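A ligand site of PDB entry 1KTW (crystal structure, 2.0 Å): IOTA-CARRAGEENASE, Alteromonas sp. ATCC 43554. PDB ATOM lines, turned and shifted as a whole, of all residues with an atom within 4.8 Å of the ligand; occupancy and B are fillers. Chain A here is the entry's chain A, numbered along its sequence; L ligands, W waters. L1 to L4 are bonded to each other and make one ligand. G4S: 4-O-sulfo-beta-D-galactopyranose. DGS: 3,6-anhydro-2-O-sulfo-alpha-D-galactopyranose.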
ATOM      1  N   PHE A 189      -2.911  -7.375  17.005  1.00  0.00           N
ATOM      2  CA  PHE A 189      -2.224  -6.516  17.978  1.00  0.00           C
ATOM      3  C   PHE A 189      -2.214  -4.993  17.758  1.00  0.00           C
ATOM      4  O   PHE A 189      -2.294  -4.232  18.716  1.00  0.00           O
ATOM      5  CB  PHE A 189      -0.761  -6.966  18.184  1.00  0.00           C
ATOM      6  CG  PHE A 189       0.133  -6.669  17.021  1.00  0.00           C
ATOM      7  CD1 PHE A 189       0.146  -7.485  15.894  1.00  0.00           C
ATOM      8  CD2 PHE A 189       0.962  -5.539  17.034  1.00  0.00           C
ATOM      9  CE1 PHE A 189       0.962  -7.185  14.795  1.00  0.00           C
ATOM     10  CE2 PHE A 189       1.773  -5.218  15.947  1.00  0.00           C
ATOM     11  CZ  PHE A 189       1.777  -6.048  14.824  1.00  0.00           C
ATOM     12  N   GLY A 190      -2.120  -4.542  16.508  1.00  0.00           N
ATOM     13  CA  GLY A 190      -2.063  -3.120  16.237  1.00  0.00           C
ATOM     14  C   GLY A 190      -3.385  -2.366  16.290  1.00  0.00           C
ATOM     15  O   GLY A 190      -3.409  -1.134  16.111  1.00  0.00           O
ATOM     16  N   ARG A 216      -8.344   2.588  22.750  1.00  0.00           N
ATOM     17  CA  ARG A 216      -7.093   3.157  22.216  1.00  0.00           C
ATOM     18  C   ARG A 216      -7.260   4.644  21.876  1.00  0.00           C
ATOM     19  O   ARG A 216      -7.767   4.975  20.815  1.00  0.00           O
ATOM     20  CB  ARG A 216      -6.675   2.351  20.967  1.00  0.00           C
ATOM     21  CG  ARG A 216      -5.374   2.781  20.249  1.00  0.00           C
ATOM     22  CD  ARG A 216      -5.216   2.057  18.869  1.00  0.00           C
ATOM     23  NE  ARG A 216      -4.889   0.624  19.005  1.00  0.00           N
ATOM     24  CZ  ARG A 216      -3.646   0.135  19.057  1.00  0.00           C
ATOM     25  NH1 ARG A 216      -2.583   0.941  18.995  1.00  0.00           N
ATOM     26  NH2 ARG A 216      -3.466  -1.176  19.171  1.00  0.00           N
ATOM     27  N   GLU A 218      -5.411   7.029  20.681  1.00  0.00           N
ATOM     28  CA  GLU A 218      -4.219   7.354  19.904  1.00  0.00           C
ATOM     29  C   GLU A 218      -4.669   8.237  18.747  1.00  0.00           C
ATOM     30  O   GLU A 218      -5.139   7.764  17.704  1.00  0.00           O
ATOM     31  CB  GLU A 218      -3.565   6.043  19.404  1.00  0.00           C
ATOM     32  CG  GLU A 218      -2.191   6.206  18.748  1.00  0.00           C
ATOM     33  CD  GLU A 218      -1.523   4.882  18.411  1.00  0.00           C
ATOM     34  OE1 GLU A 218      -2.224   3.847  18.313  1.00  0.00           O
ATOM     35  OE2 GLU A 218      -0.290   4.854  18.220  1.00  0.00           O
ATOM     36  N   ASP A 220      -3.909  10.133  15.853  1.00  0.00           N
ATOM     37  CA  ASP A 220      -2.936  10.380  14.789  1.00  0.00           C
ATOM     38  C   ASP A 220      -3.389  10.494  13.322  1.00  0.00           C
ATOM     39  O   ASP A 220      -2.572  10.327  12.413  1.00  0.00           O
ATOM     40  CB  ASP A 220      -1.833   9.309  14.878  1.00  0.00           C
ATOM     41  CG  ASP A 220      -2.347   7.909  14.589  1.00  0.00           C
ATOM     42  OD1 ASP A 220      -3.564   7.737  14.348  1.00  0.00           O
ATOM     43  OD2 ASP A 220      -1.533   6.956  14.593  1.00  0.00           O
ATOM     44  N   LEU A 246      -2.364  -6.100  24.475  1.00  0.00           N
ATOM     45  CA  LEU A 246      -1.380  -5.083  24.858  1.00  0.00           C
ATOM     46  C   LEU A 246      -1.768  -4.343  26.142  1.00  0.00           C
ATOM     47  O   LEU A 246      -0.959  -4.240  27.095  1.00  0.00           O
ATOM     48  CB  LEU A 246      -1.207  -4.037  23.723  1.00  0.00           C
ATOM     49  CG  LEU A 246      -0.562  -4.393  22.377  1.00  0.00           C
ATOM     50  CD1 LEU A 246      -0.735  -3.212  21.397  1.00  0.00           C
ATOM     51  CD2 LEU A 246       0.919  -4.724  22.588  1.00  0.00           C
ATOM     52  N   HIS A 254       0.540  11.535  19.926  1.00  0.00           N
ATOM     53  CA  HIS A 254       1.308  11.869  18.725  1.00  0.00           C
ATOM     54  C   HIS A 254       1.537  13.395  18.680  1.00  0.00           C
ATOM     55  O   HIS A 254       2.140  13.942  19.609  1.00  0.00           O
ATOM     56  CB  HIS A 254       0.587  11.340  17.455  1.00  0.00           C
ATOM     57  CG  HIS A 254       0.630   9.847  17.310  1.00  0.00           C
ATOM     58  ND1 HIS A 254       1.264   9.220  16.258  1.00  0.00           N
ATOM     59  CD2 HIS A 254       0.160   8.856  18.114  1.00  0.00           C
ATOM     60  CE1 HIS A 254       1.174   7.902  16.407  1.00  0.00           C
ATOM     61  NE2 HIS A 254       0.505   7.658  17.515  1.00  0.00           N
ATOM     62  N   ARG A 276      -1.562   1.934  29.715  1.00  0.00           N
ATOM     63  CA  ARG A 276      -0.346   2.340  29.012  1.00  0.00           C
ATOM     64  C   ARG A 276      -0.433   3.806  28.532  1.00  0.00           C
ATOM     65  O   ARG A 276      -1.460   4.227  28.004  1.00  0.00           O
ATOM     66  CB  ARG A 276      -0.092   1.429  27.786  1.00  0.00           C
ATOM     67  CG  ARG A 276       0.973   1.952  26.801  1.00  0.00           C
ATOM     68  CD  ARG A 276       1.224   0.939  25.637  1.00  0.00           C
ATOM     69  NE  ARG A 276       1.824   1.587  24.464  1.00  0.00           N
ATOM     70  CZ  ARG A 276       1.980   1.005  23.268  1.00  0.00           C
ATOM     71  NH1 ARG A 276       1.602  -0.257  23.064  1.00  0.00           N
ATOM     72  NH2 ARG A 276       2.495   1.709  22.264  1.00  0.00           N
ATOM     73  N   ASP A 278       1.907   6.726  26.304  1.00  0.00           N
ATOM     74  CA  ASP A 278       3.066   7.006  25.453  1.00  0.00           C
ATOM     75  C   ASP A 278       3.362   8.520  25.426  1.00  0.00           C
ATOM     76  O   ASP A 278       2.463   9.352  25.620  1.00  0.00           O
ATOM     77  CB  ASP A 278       2.826   6.569  23.990  1.00  0.00           C
ATOM     78  CG  ASP A 278       2.802   5.046  23.792  1.00  0.00           C
ATOM     79  OD1 ASP A 278       2.959   4.277  24.759  1.00  0.00           O
ATOM     80  OD2 ASP A 278       2.602   4.611  22.633  1.00  0.00           O
ATOM     81  N   ARG A 294      15.402   2.944   4.214  1.00  0.00           N
ATOM     82  CA  ARG A 294      15.488   3.221   5.643  1.00  0.00           C
ATOM     83  C   ARG A 294      16.432   4.393   5.870  1.00  0.00           C
ATOM     84  O   ARG A 294      16.024   5.465   6.310  1.00  0.00           O
ATOM     85  CB  ARG A 294      16.016   1.991   6.404  1.00  0.00           C
ATOM     86  CG  ARG A 294      16.337   2.254   7.858  1.00  0.00           C
ATOM     87  CD  ARG A 294      15.238   1.721   8.748  1.00  0.00           C
ATOM     88  NE  ARG A 294      15.241   0.261   8.768  1.00  0.00           N
ATOM     89  CZ  ARG A 294      14.170  -0.487   9.028  1.00  0.00           C
ATOM     90  NH1 ARG A 294      13.017   0.080   9.281  1.00  0.00           N
ATOM     91  NH2 ARG A 294      14.272  -1.811   9.031  1.00  0.00           N
ATOM     92  N   THR A 312      15.947   6.069  14.185  1.00  0.00           N
ATOM     93  CA  THR A 312      15.903   5.129  13.067  1.00  0.00           C
ATOM     94  C   THR A 312      14.456   4.970  12.592  1.00  0.00           C
ATOM     95  O   THR A 312      13.560   4.670  13.377  1.00  0.00           O
ATOM     96  CB  THR A 312      16.448   3.732  13.471  1.00  0.00           C
ATOM     97  OG1 THR A 312      17.783   3.854  13.976  1.00  0.00           O
ATOM     98  CG2 THR A 312      16.471   2.805  12.248  1.00  0.00           C
ATOM     99  N   TYR A 314      11.017   3.541  10.749  1.00  0.00           N
ATOM    100  CA  TYR A 314      10.375   2.232  10.729  1.00  0.00           C
ATOM    101  C   TYR A 314       9.193   2.215   9.747  1.00  0.00           C
ATOM    102  O   TYR A 314       8.652   3.263   9.392  1.00  0.00           O
ATOM    103  CB  TYR A 314       9.917   1.824  12.146  1.00  0.00           C
ATOM    104  CG  TYR A 314       8.798   2.647  12.757  1.00  0.00           C
ATOM    105  CD1 TYR A 314       7.461   2.319  12.518  1.00  0.00           C
ATOM    106  CD2 TYR A 314       9.078   3.747  13.574  1.00  0.00           C
ATOM    107  CE1 TYR A 314       6.426   3.061  13.099  1.00  0.00           C
ATOM    108  CE2 TYR A 314       8.043   4.489  14.155  1.00  0.00           C
ATOM    109  CZ  TYR A 314       6.722   4.146  13.906  1.00  0.00           C
ATOM    110  OH  TYR A 314       5.688   4.874  14.469  1.00  0.00           O
ATOM    111  N   ALA A 315       8.818   1.024   9.308  1.00  0.00           N
ATOM    112  CA  ALA A 315       7.722   0.860   8.364  1.00  0.00           C
ATOM    113  C   ALA A 315       6.405   1.363   8.914  1.00  0.00           C
ATOM    114  O   ALA A 315       5.799   0.726   9.779  1.00  0.00           O
ATOM    115  CB  ALA A 315       7.599  -0.602   7.973  1.00  0.00           C
ATOM    116  N   TRP A 323       7.596   4.953   5.243  1.00  0.00           N
ATOM    117  CA  TRP A 323       8.581   5.077   6.315  1.00  0.00           C
ATOM    118  C   TRP A 323       8.295   6.255   7.232  1.00  0.00           C
ATOM    119  O   TRP A 323       8.067   7.380   6.772  1.00  0.00           O
ATOM    120  CB  TRP A 323       9.980   5.235   5.743  1.00  0.00           C
ATOM    121  CG  TRP A 323      10.429   4.081   4.905  1.00  0.00           C
ATOM    122  CD1 TRP A 323      10.389   3.969   3.542  1.00  0.00           C
ATOM    123  CD2 TRP A 323      10.972   2.845   5.394  1.00  0.00           C
ATOM    124  NE1 TRP A 323      10.875   2.750   3.146  1.00  0.00           N
ATOM    125  CE2 TRP A 323      11.237   2.036   4.259  1.00  0.00           C
ATOM    126  CE3 TRP A 323      11.251   2.343   6.668  1.00  0.00           C
ATOM    127  CZ2 TRP A 323      11.779   0.748   4.376  1.00  0.00           C
ATOM    128  CZ3 TRP A 323      11.790   1.062   6.779  1.00  0.00           C
ATOM    129  CH2 TRP A 323      12.049   0.283   5.633  1.00  0.00           C
ATOM    130  N   ARG A 326      10.872   9.330  13.519  1.00  0.00           N
ATOM    131  CA  ARG A 326      10.511  10.028  14.753  1.00  0.00           C
ATOM    132  C   ARG A 326      11.652  10.942  15.193  1.00  0.00           C
ATOM    133  O   ARG A 326      12.795  10.513  15.308  1.00  0.00           O
ATOM    134  CB  ARG A 326      10.174   9.000  15.845  1.00  0.00           C
ATOM    135  CG  ARG A 326       9.494   9.574  17.077  1.00  0.00           C
ATOM    136  CD  ARG A 326       9.122   8.472  18.095  1.00  0.00           C
ATOM    137  NE  ARG A 326       8.072   7.576  17.611  1.00  0.00           N
ATOM    138  CZ  ARG A 326       7.506   6.614  18.350  1.00  0.00           C
ATOM    139  NH1 ARG A 326       7.890   6.426  19.606  1.00  0.00           N
ATOM    140  NH2 ARG A 326       6.571   5.825  17.838  1.00  0.00           N
ATOM    141  N   LYS A 367       5.733  -5.606  22.852  1.00  0.00           N
ATOM    142  CA  LYS A 367       6.515  -4.868  21.866  1.00  0.00           C
ATOM    143  C   LYS A 367       8.017  -5.138  22.126  1.00  0.00           C
ATOM    144  O   LYS A 367       8.396  -5.463  23.245  1.00  0.00           O
ATOM    145  CB  LYS A 367       6.260  -3.355  21.965  1.00  0.00           C
ATOM    146  CG  LYS A 367       4.785  -2.947  21.780  1.00  0.00           C
ATOM    147  CD  LYS A 367       4.259  -3.271  20.377  1.00  0.00           C
ATOM    148  CE  LYS A 367       4.877  -2.366  19.317  1.00  0.00           C
ATOM    149  NZ  LYS A 367       4.334  -2.675  17.941  1.00  0.00           N
ATOM    150  N   GLN A 368       8.850  -4.983  21.105  1.00  0.00           N
ATOM    151  CA  GLN A 368      10.285  -5.238  21.232  1.00  0.00           C
ATOM    152  C   GLN A 368      10.951  -4.315  22.264  1.00  0.00           C
ATOM    153  O   GLN A 368      11.797  -4.755  23.020  1.00  0.00           O
ATOM    154  CB  GLN A 368      10.990  -5.080  19.876  1.00  0.00           C
ATOM    155  CG  GLN A 368      12.342  -5.819  19.775  1.00  0.00           C
ATOM    156  CD  GLN A 368      13.092  -5.509  18.485  1.00  0.00           C
ATOM    157  OE1 GLN A 368      13.707  -4.449  18.356  1.00  0.00           O
ATOM    158  NE2 GLN A 368      13.034  -6.404  17.517  1.00  0.00           N
ATOM    159  N   ASP A 369      10.562  -3.039  22.270  1.00  0.00           N
ATOM    160  CA  ASP A 369      11.130  -2.080  23.213  1.00  0.00           C
ATOM    161  C   ASP A 369      10.673  -2.291  24.658  1.00  0.00           C
ATOM    162  O   ASP A 369      10.985  -1.471  25.529  1.00  0.00           O
ATOM    163  CB  ASP A 369      10.758  -0.643  22.784  1.00  0.00           C
ATOM    164  CG  ASP A 369      11.524  -0.187  21.551  1.00  0.00           C
ATOM    165  OD1 ASP A 369      11.437  -0.866  20.500  1.00  0.00           O
ATOM    166  OD2 ASP A 369      12.205   0.863  21.613  1.00  0.00           O
ATOM    167  N   LYS A 394       6.211  -8.598   9.228  1.00  0.00           N
ATOM    168  CA  LYS A 394       7.157  -7.611   9.746  1.00  0.00           C
ATOM    169  C   LYS A 394       7.647  -8.078  11.120  1.00  0.00           C
ATOM    170  O   LYS A 394       7.157  -7.622  12.151  1.00  0.00           O
ATOM    171  CB  LYS A 394       6.490  -6.245   9.847  1.00  0.00           C
ATOM    172  CG  LYS A 394       5.937  -5.740   8.520  1.00  0.00           C
ATOM    173  CD  LYS A 394       5.150  -4.461   8.678  1.00  0.00           C
ATOM    174  CE  LYS A 394       4.469  -4.071   7.378  1.00  0.00           C
ATOM    175  NZ  LYS A 394       3.612  -2.858   7.540  1.00  0.00           N
ATOM    176  N   GLN A 395       8.627  -8.984  11.128  1.00  0.00           N
ATOM    177  CA  GLN A 395       9.147  -9.520  12.381  1.00  0.00           C
ATOM    178  C   GLN A 395       9.785  -8.463  13.257  1.00  0.00           C
ATOM    179  O   GLN A 395      10.609  -7.673  12.791  1.00  0.00           O
ATOM    180  CB  GLN A 395      10.137 -10.672  12.105  1.00  0.00           C
ATOM    181  CG  GLN A 395       9.460 -11.927  11.510  1.00  0.00           C
ATOM    182  CD  GLN A 395      10.337 -13.176  11.581  1.00  0.00           C
ATOM    183  OE1 GLN A 395      11.457 -13.188  11.079  1.00  0.00           O
ATOM    184  NE2 GLN A 395       9.804 -14.228  12.204  1.00  0.00           N
ATOM    185  N   GLY A 396       9.399  -8.453  14.534  1.00  0.00           N
ATOM    186  CA  GLY A 396       9.912  -7.476  15.479  1.00  0.00           C
ATOM    187  C   GLY A 396       8.822  -6.530  15.973  1.00  0.00           C
ATOM    188  O   GLY A 396       8.965  -5.884  17.022  1.00  0.00           O
ATOM    189  N   GLN A 397       7.721  -6.438  15.221  1.00  0.00           N
ATOM    190  CA  GLN A 397       6.608  -5.565  15.601  1.00  0.00           C
ATOM    191  C   GLN A 397       5.744  -6.182  16.717  1.00  0.00           C
ATOM    192  O   GLN A 397       5.052  -5.457  17.448  1.00  0.00           O
ATOM    193  CB  GLN A 397       5.702  -5.264  14.379  1.00  0.00           C
ATOM    194  CG  GLN A 397       6.371  -4.480  13.256  1.00  0.00           C
ATOM    195  CD  GLN A 397       5.361  -3.861  12.271  1.00  0.00           C
ATOM    196  OE1 GLN A 397       4.309  -4.445  11.980  1.00  0.00           O
ATOM    197  NE2 GLN A 397       5.696  -2.687  11.739  1.00  0.00           N
ATOM    198  N   TYR A 452      15.671 -11.812  17.357  1.00  0.00           N
ATOM    199  CA  TYR A 452      15.322 -12.470  16.116  1.00  0.00           C
ATOM    200  C   TYR A 452      15.671 -13.968  16.037  1.00  0.00           C
ATOM    201  O   TYR A 452      15.263 -14.646  15.092  1.00  0.00           O
ATOM    202  CB  TYR A 452      15.977 -11.699  14.951  1.00  0.00           C
ATOM    203  CG  TYR A 452      15.482 -10.264  14.825  1.00  0.00           C
ATOM    204  CD1 TYR A 452      14.191  -9.992  14.351  1.00  0.00           C
ATOM    205  CD2 TYR A 452      16.274  -9.187  15.234  1.00  0.00           C
ATOM    206  CE1 TYR A 452      13.700  -8.673  14.280  1.00  0.00           C
ATOM    207  CE2 TYR A 452      15.790  -7.869  15.175  1.00  0.00           C
ATOM    208  CZ  TYR A 452      14.507  -7.626  14.695  1.00  0.00           C
ATOM    209  OH  TYR A 452      14.029  -6.336  14.648  1.00  0.00           O
HETATM  210  C1  G4S L   1      17.182  -2.666  13.731  1.00  0.00           C
HETATM  211  C2  G4S L   1      15.818  -2.213  13.238  1.00  0.00           C
HETATM  212  C3  G4S L   1      14.848  -3.374  13.363  1.00  0.00           C
HETATM  213  C4  G4S L   1      15.377  -4.592  12.605  1.00  0.00           C
HETATM  214  C5  G4S L   1      16.757  -4.941  13.137  1.00  0.00           C
HETATM  215  C6  G4S L   1      17.400  -6.088  12.391  1.00  0.00           C
HETATM  216  O1  G4S L   1      18.097  -1.643  13.563  1.00  0.00           O
HETATM  217  O2  G4S L   1      15.358  -1.119  14.004  1.00  0.00           O
HETATM  218  O3  G4S L   1      13.575  -2.967  12.831  1.00  0.00           O
HETATM  219  O4  G4S L   1      15.450  -4.318  11.193  1.00  0.00           O
HETATM  220  O5  G4S L   1      17.629  -3.802  12.986  1.00  0.00           O
HETATM  221  O6  G4S L   1      18.816  -6.081  12.587  1.00  0.00           O
HETATM  222  S   G4S L   1      14.567  -5.252  10.247  1.00  0.00           S
HETATM  223  O7  G4S L   1      14.460  -4.624   8.921  1.00  0.00           O
HETATM  224  O8  G4S L   1      13.221  -5.393  10.830  1.00  0.00           O
HETATM  225  O9  G4S L   1      15.192  -6.581  10.132  1.00  0.00           O
HETATM  226  C1  DGS L   2      12.505  -3.188  13.690  1.00  0.00           C
HETATM  227  C2  DGS L   2      11.231  -3.353  12.859  1.00  0.00           C
HETATM  228  C3  DGS L   2      10.029  -3.378  13.817  1.00  0.00           C
HETATM  229  C4  DGS L   2       9.963  -2.052  14.564  1.00  0.00           C
HETATM  230  C5  DGS L   2      11.153  -2.261  15.495  1.00  0.00           C
HETATM  231  C6  DGS L   2      10.946  -3.729  15.908  1.00  0.00           C
HETATM  232  O2  DGS L   2      11.163  -2.326  11.848  1.00  0.00           O
HETATM  233  O3  DGS L   2      10.284  -4.394  14.809  1.00  0.00           O
HETATM  234  O4  DGS L   2       8.716  -1.976  15.301  1.00  0.00           O
HETATM  235  O5  DGS L   2      12.364  -2.155  14.685  1.00  0.00           O
HETATM  236  O7  DGS L   2       9.872  -1.093  10.090  1.00  0.00           O
HETATM  237  O8  DGS L   2       8.651  -2.545  11.600  1.00  0.00           O
HETATM  238  O9  DGS L   2      10.040  -3.492   9.919  1.00  0.00           O
HETATM  239  S   DGS L   2       9.907  -2.351  10.842  1.00  0.00           S
HETATM  240  C1  G4S L   3       8.097  -0.726  15.431  1.00  0.00           C
HETATM  241  C2  G4S L   3       6.756  -0.894  16.182  1.00  0.00           C
HETATM  242  C3  G4S L   3       6.160   0.492  16.440  1.00  0.00           C
HETATM  243  C4  G4S L   3       7.147   1.340  17.254  1.00  0.00           C
HETATM  244  C5  G4S L   3       8.439   1.463  16.422  1.00  0.00           C
HETATM  245  C6  G4S L   3       9.555   2.250  17.123  1.00  0.00           C
HETATM  246  O2  G4S L   3       5.843  -1.676  15.412  1.00  0.00           O
HETATM  247  O3  G4S L   3       4.912   0.357  17.131  1.00  0.00           O
HETATM  248  O4  G4S L   3       7.493   0.680  18.495  1.00  0.00           O
HETATM  249  O5  G4S L   3       8.983   0.129  16.190  1.00  0.00           O
HETATM  250  O6  G4S L   3       9.128   3.537  17.538  1.00  0.00           O
HETATM  251  S   G4S L   3       6.978   1.339  19.865  1.00  0.00           S
HETATM  252  O7  G4S L   3       7.308   0.436  20.977  1.00  0.00           O
HETATM  253  O8  G4S L   3       5.547   1.656  19.781  1.00  0.00           O
HETATM  254  O9  G4S L   3       7.667   2.620  20.044  1.00  0.00           O
HETATM  255  C1  DGS L   4       4.098   1.488  17.114  1.00  0.00           C
HETATM  256  C2  DGS L   4       2.878   1.196  18.000  1.00  0.00           C
HETATM  257  C3  DGS L   4       1.806   2.270  17.745  1.00  0.00           C
HETATM  258  C4  DGS L   4       1.393   2.268  16.296  1.00  0.00           C
HETATM  259  C5  DGS L   4       2.648   2.860  15.688  1.00  0.00           C
HETATM  260  C6  DGS L   4       2.923   3.997  16.691  1.00  0.00           C
HETATM  261  O2  DGS L   4       2.482  -0.194  17.831  1.00  0.00           O
HETATM  262  O3  DGS L   4       2.444   3.545  17.978  1.00  0.00           O
HETATM  263  O4  DGS L   4       0.290   3.150  16.121  1.00  0.00           O
HETATM  264  O5  DGS L   4       3.703   1.856  15.768  1.00  0.00           O
HETATM  265  O7  DGS L   4       1.103  -2.216  18.379  1.00  0.00           O
HETATM  266  O8  DGS L   4       0.111   0.041  18.679  1.00  0.00           O
HETATM  267  O9  DGS L   4       1.735  -0.691  20.142  1.00  0.00           O
HETATM  268  S   DGS L   4       1.317  -0.801  18.730  1.00  0.00           S
HETATM  269  O   HOH W   1       4.421  -0.245  13.653  1.00  0.00           O
HETATM  270  O   HOH W   2      11.180   5.264  16.592  1.00  0.00           O
HETATM  271  O   HOH W   3       7.716   2.319  23.518  1.00  0.00           O
HETATM  272  O   HOH W   4       5.040   4.289  20.345  1.00  0.00           O
HETATM  273  O   HOH W   5       9.290  -1.728  19.750  1.00  0.00           O
HETATM  274  O   HOH W   6      16.242   0.302  16.163  1.00  0.00           O
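OE1 of Glu 218 is in salt-bridge range of NH1 of Arg 216, 3.0 Å away. OE2 of Glu 218 lies within hydrogen-bond range of NE2 of His 254 (3.0 Å). The guanidinium group (NH2) of Arg 216 sits at hydrogen-bond distance from the backbone carbonyl oxygen (O) of Phe 189, 3.3 Å away. The guanidinium group (NH2) of Arg 216 lies within hydrogen-bond range of the backbone carbonyl oxygen (O) of Gly 190, 3.1 Å away. NH2 of Arg 276 lies within salt-bridge range of OD2 of Asp 278 (2.9 Å). O of Gln 397 is in hydrogen-bond range of NZ of Lys 367 (2.9 Å). OH of Tyr 452 sits at hydrogen-bond distance from NE2 of Gln 368.
N of Ala 315 is in hydrogen-bond range of O7 of DGS L2 (2.5 Å). An oxygen (O4) of DGS L4 lies within hydrogen-bond range of the side-chain carboxylate (OE2) of Glu 218 (2.8 Å). NH2 of Arg 294 lies within salt-bridge range of O7 of G4S L1 (2.8 Å). NH1 of Arg 216 is in salt-bridge range of O8 of DGS L4 (2.9 Å). NH1 of Arg 276 lies within salt-bridge range of O9 of DGS L4, 3.0 Å away. An oxygen (O3) of DGS L2 lies within hydrogen-bond range of the backbone NH (N) of Gln 397 (3.3 Å). O8 of DGS L2 sits at hydrogen-bond distance from NE2 of Gln 397 (3.0 Å). The side-chain amino group (NZ) of Lys 367 is in salt-bridge range of an oxygen (O7) of DGS L4 (3.3 Å). O9 of G4S L3 is in salt-bridge range of NH1 of Arg 326.
An oxygen (O3) of DGS L2 sits close to the backbone carbonyl oxygen of Gly 396, at 3.0 Å. Phe 189 touches the ligand. CA of Gly 190 touches O7 of DGS L4 (3.9 Å). CD1 of Leu 246 touches O7 of DGS L4 (3.7 Å). C of Tyr 314 touches O7 of DGS L2, 3.4 Å away. Gln 368 touches the ligand. O of Gln 395 touches O3 of DGS L2 (3.9 Å). OH of Tyr 452 touches C4 of G4S L1, 3.0 Å away. Within 4 Å of the ligand: Phe 189, Gly 190, Arg 216, Glu 218, Leu 246, Arg 276, Arg 294, Tyr 314, Ala 315, Arg 326, Lys 367, Gln 368, Gln 395, Gly 396, Gln 397 and Tyr 452. Along chain A the residues within 4 Å of the ligand span positions 189 to 452.
Water W1 bridges O2 of G4S L3 and NE2 of Gln 397. Water W4 lies within hydrogen-bond range of O8 of G4S L3 (2.7 Å), NH2 of Arg 326 (3.3 Å) and OD2 of Asp 278 (3.4 Å). Water W5 lies within hydrogen-bond range of OD1 of Asp 369 (2.4 Å) and O7 of G4S L3 (3.2 Å).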
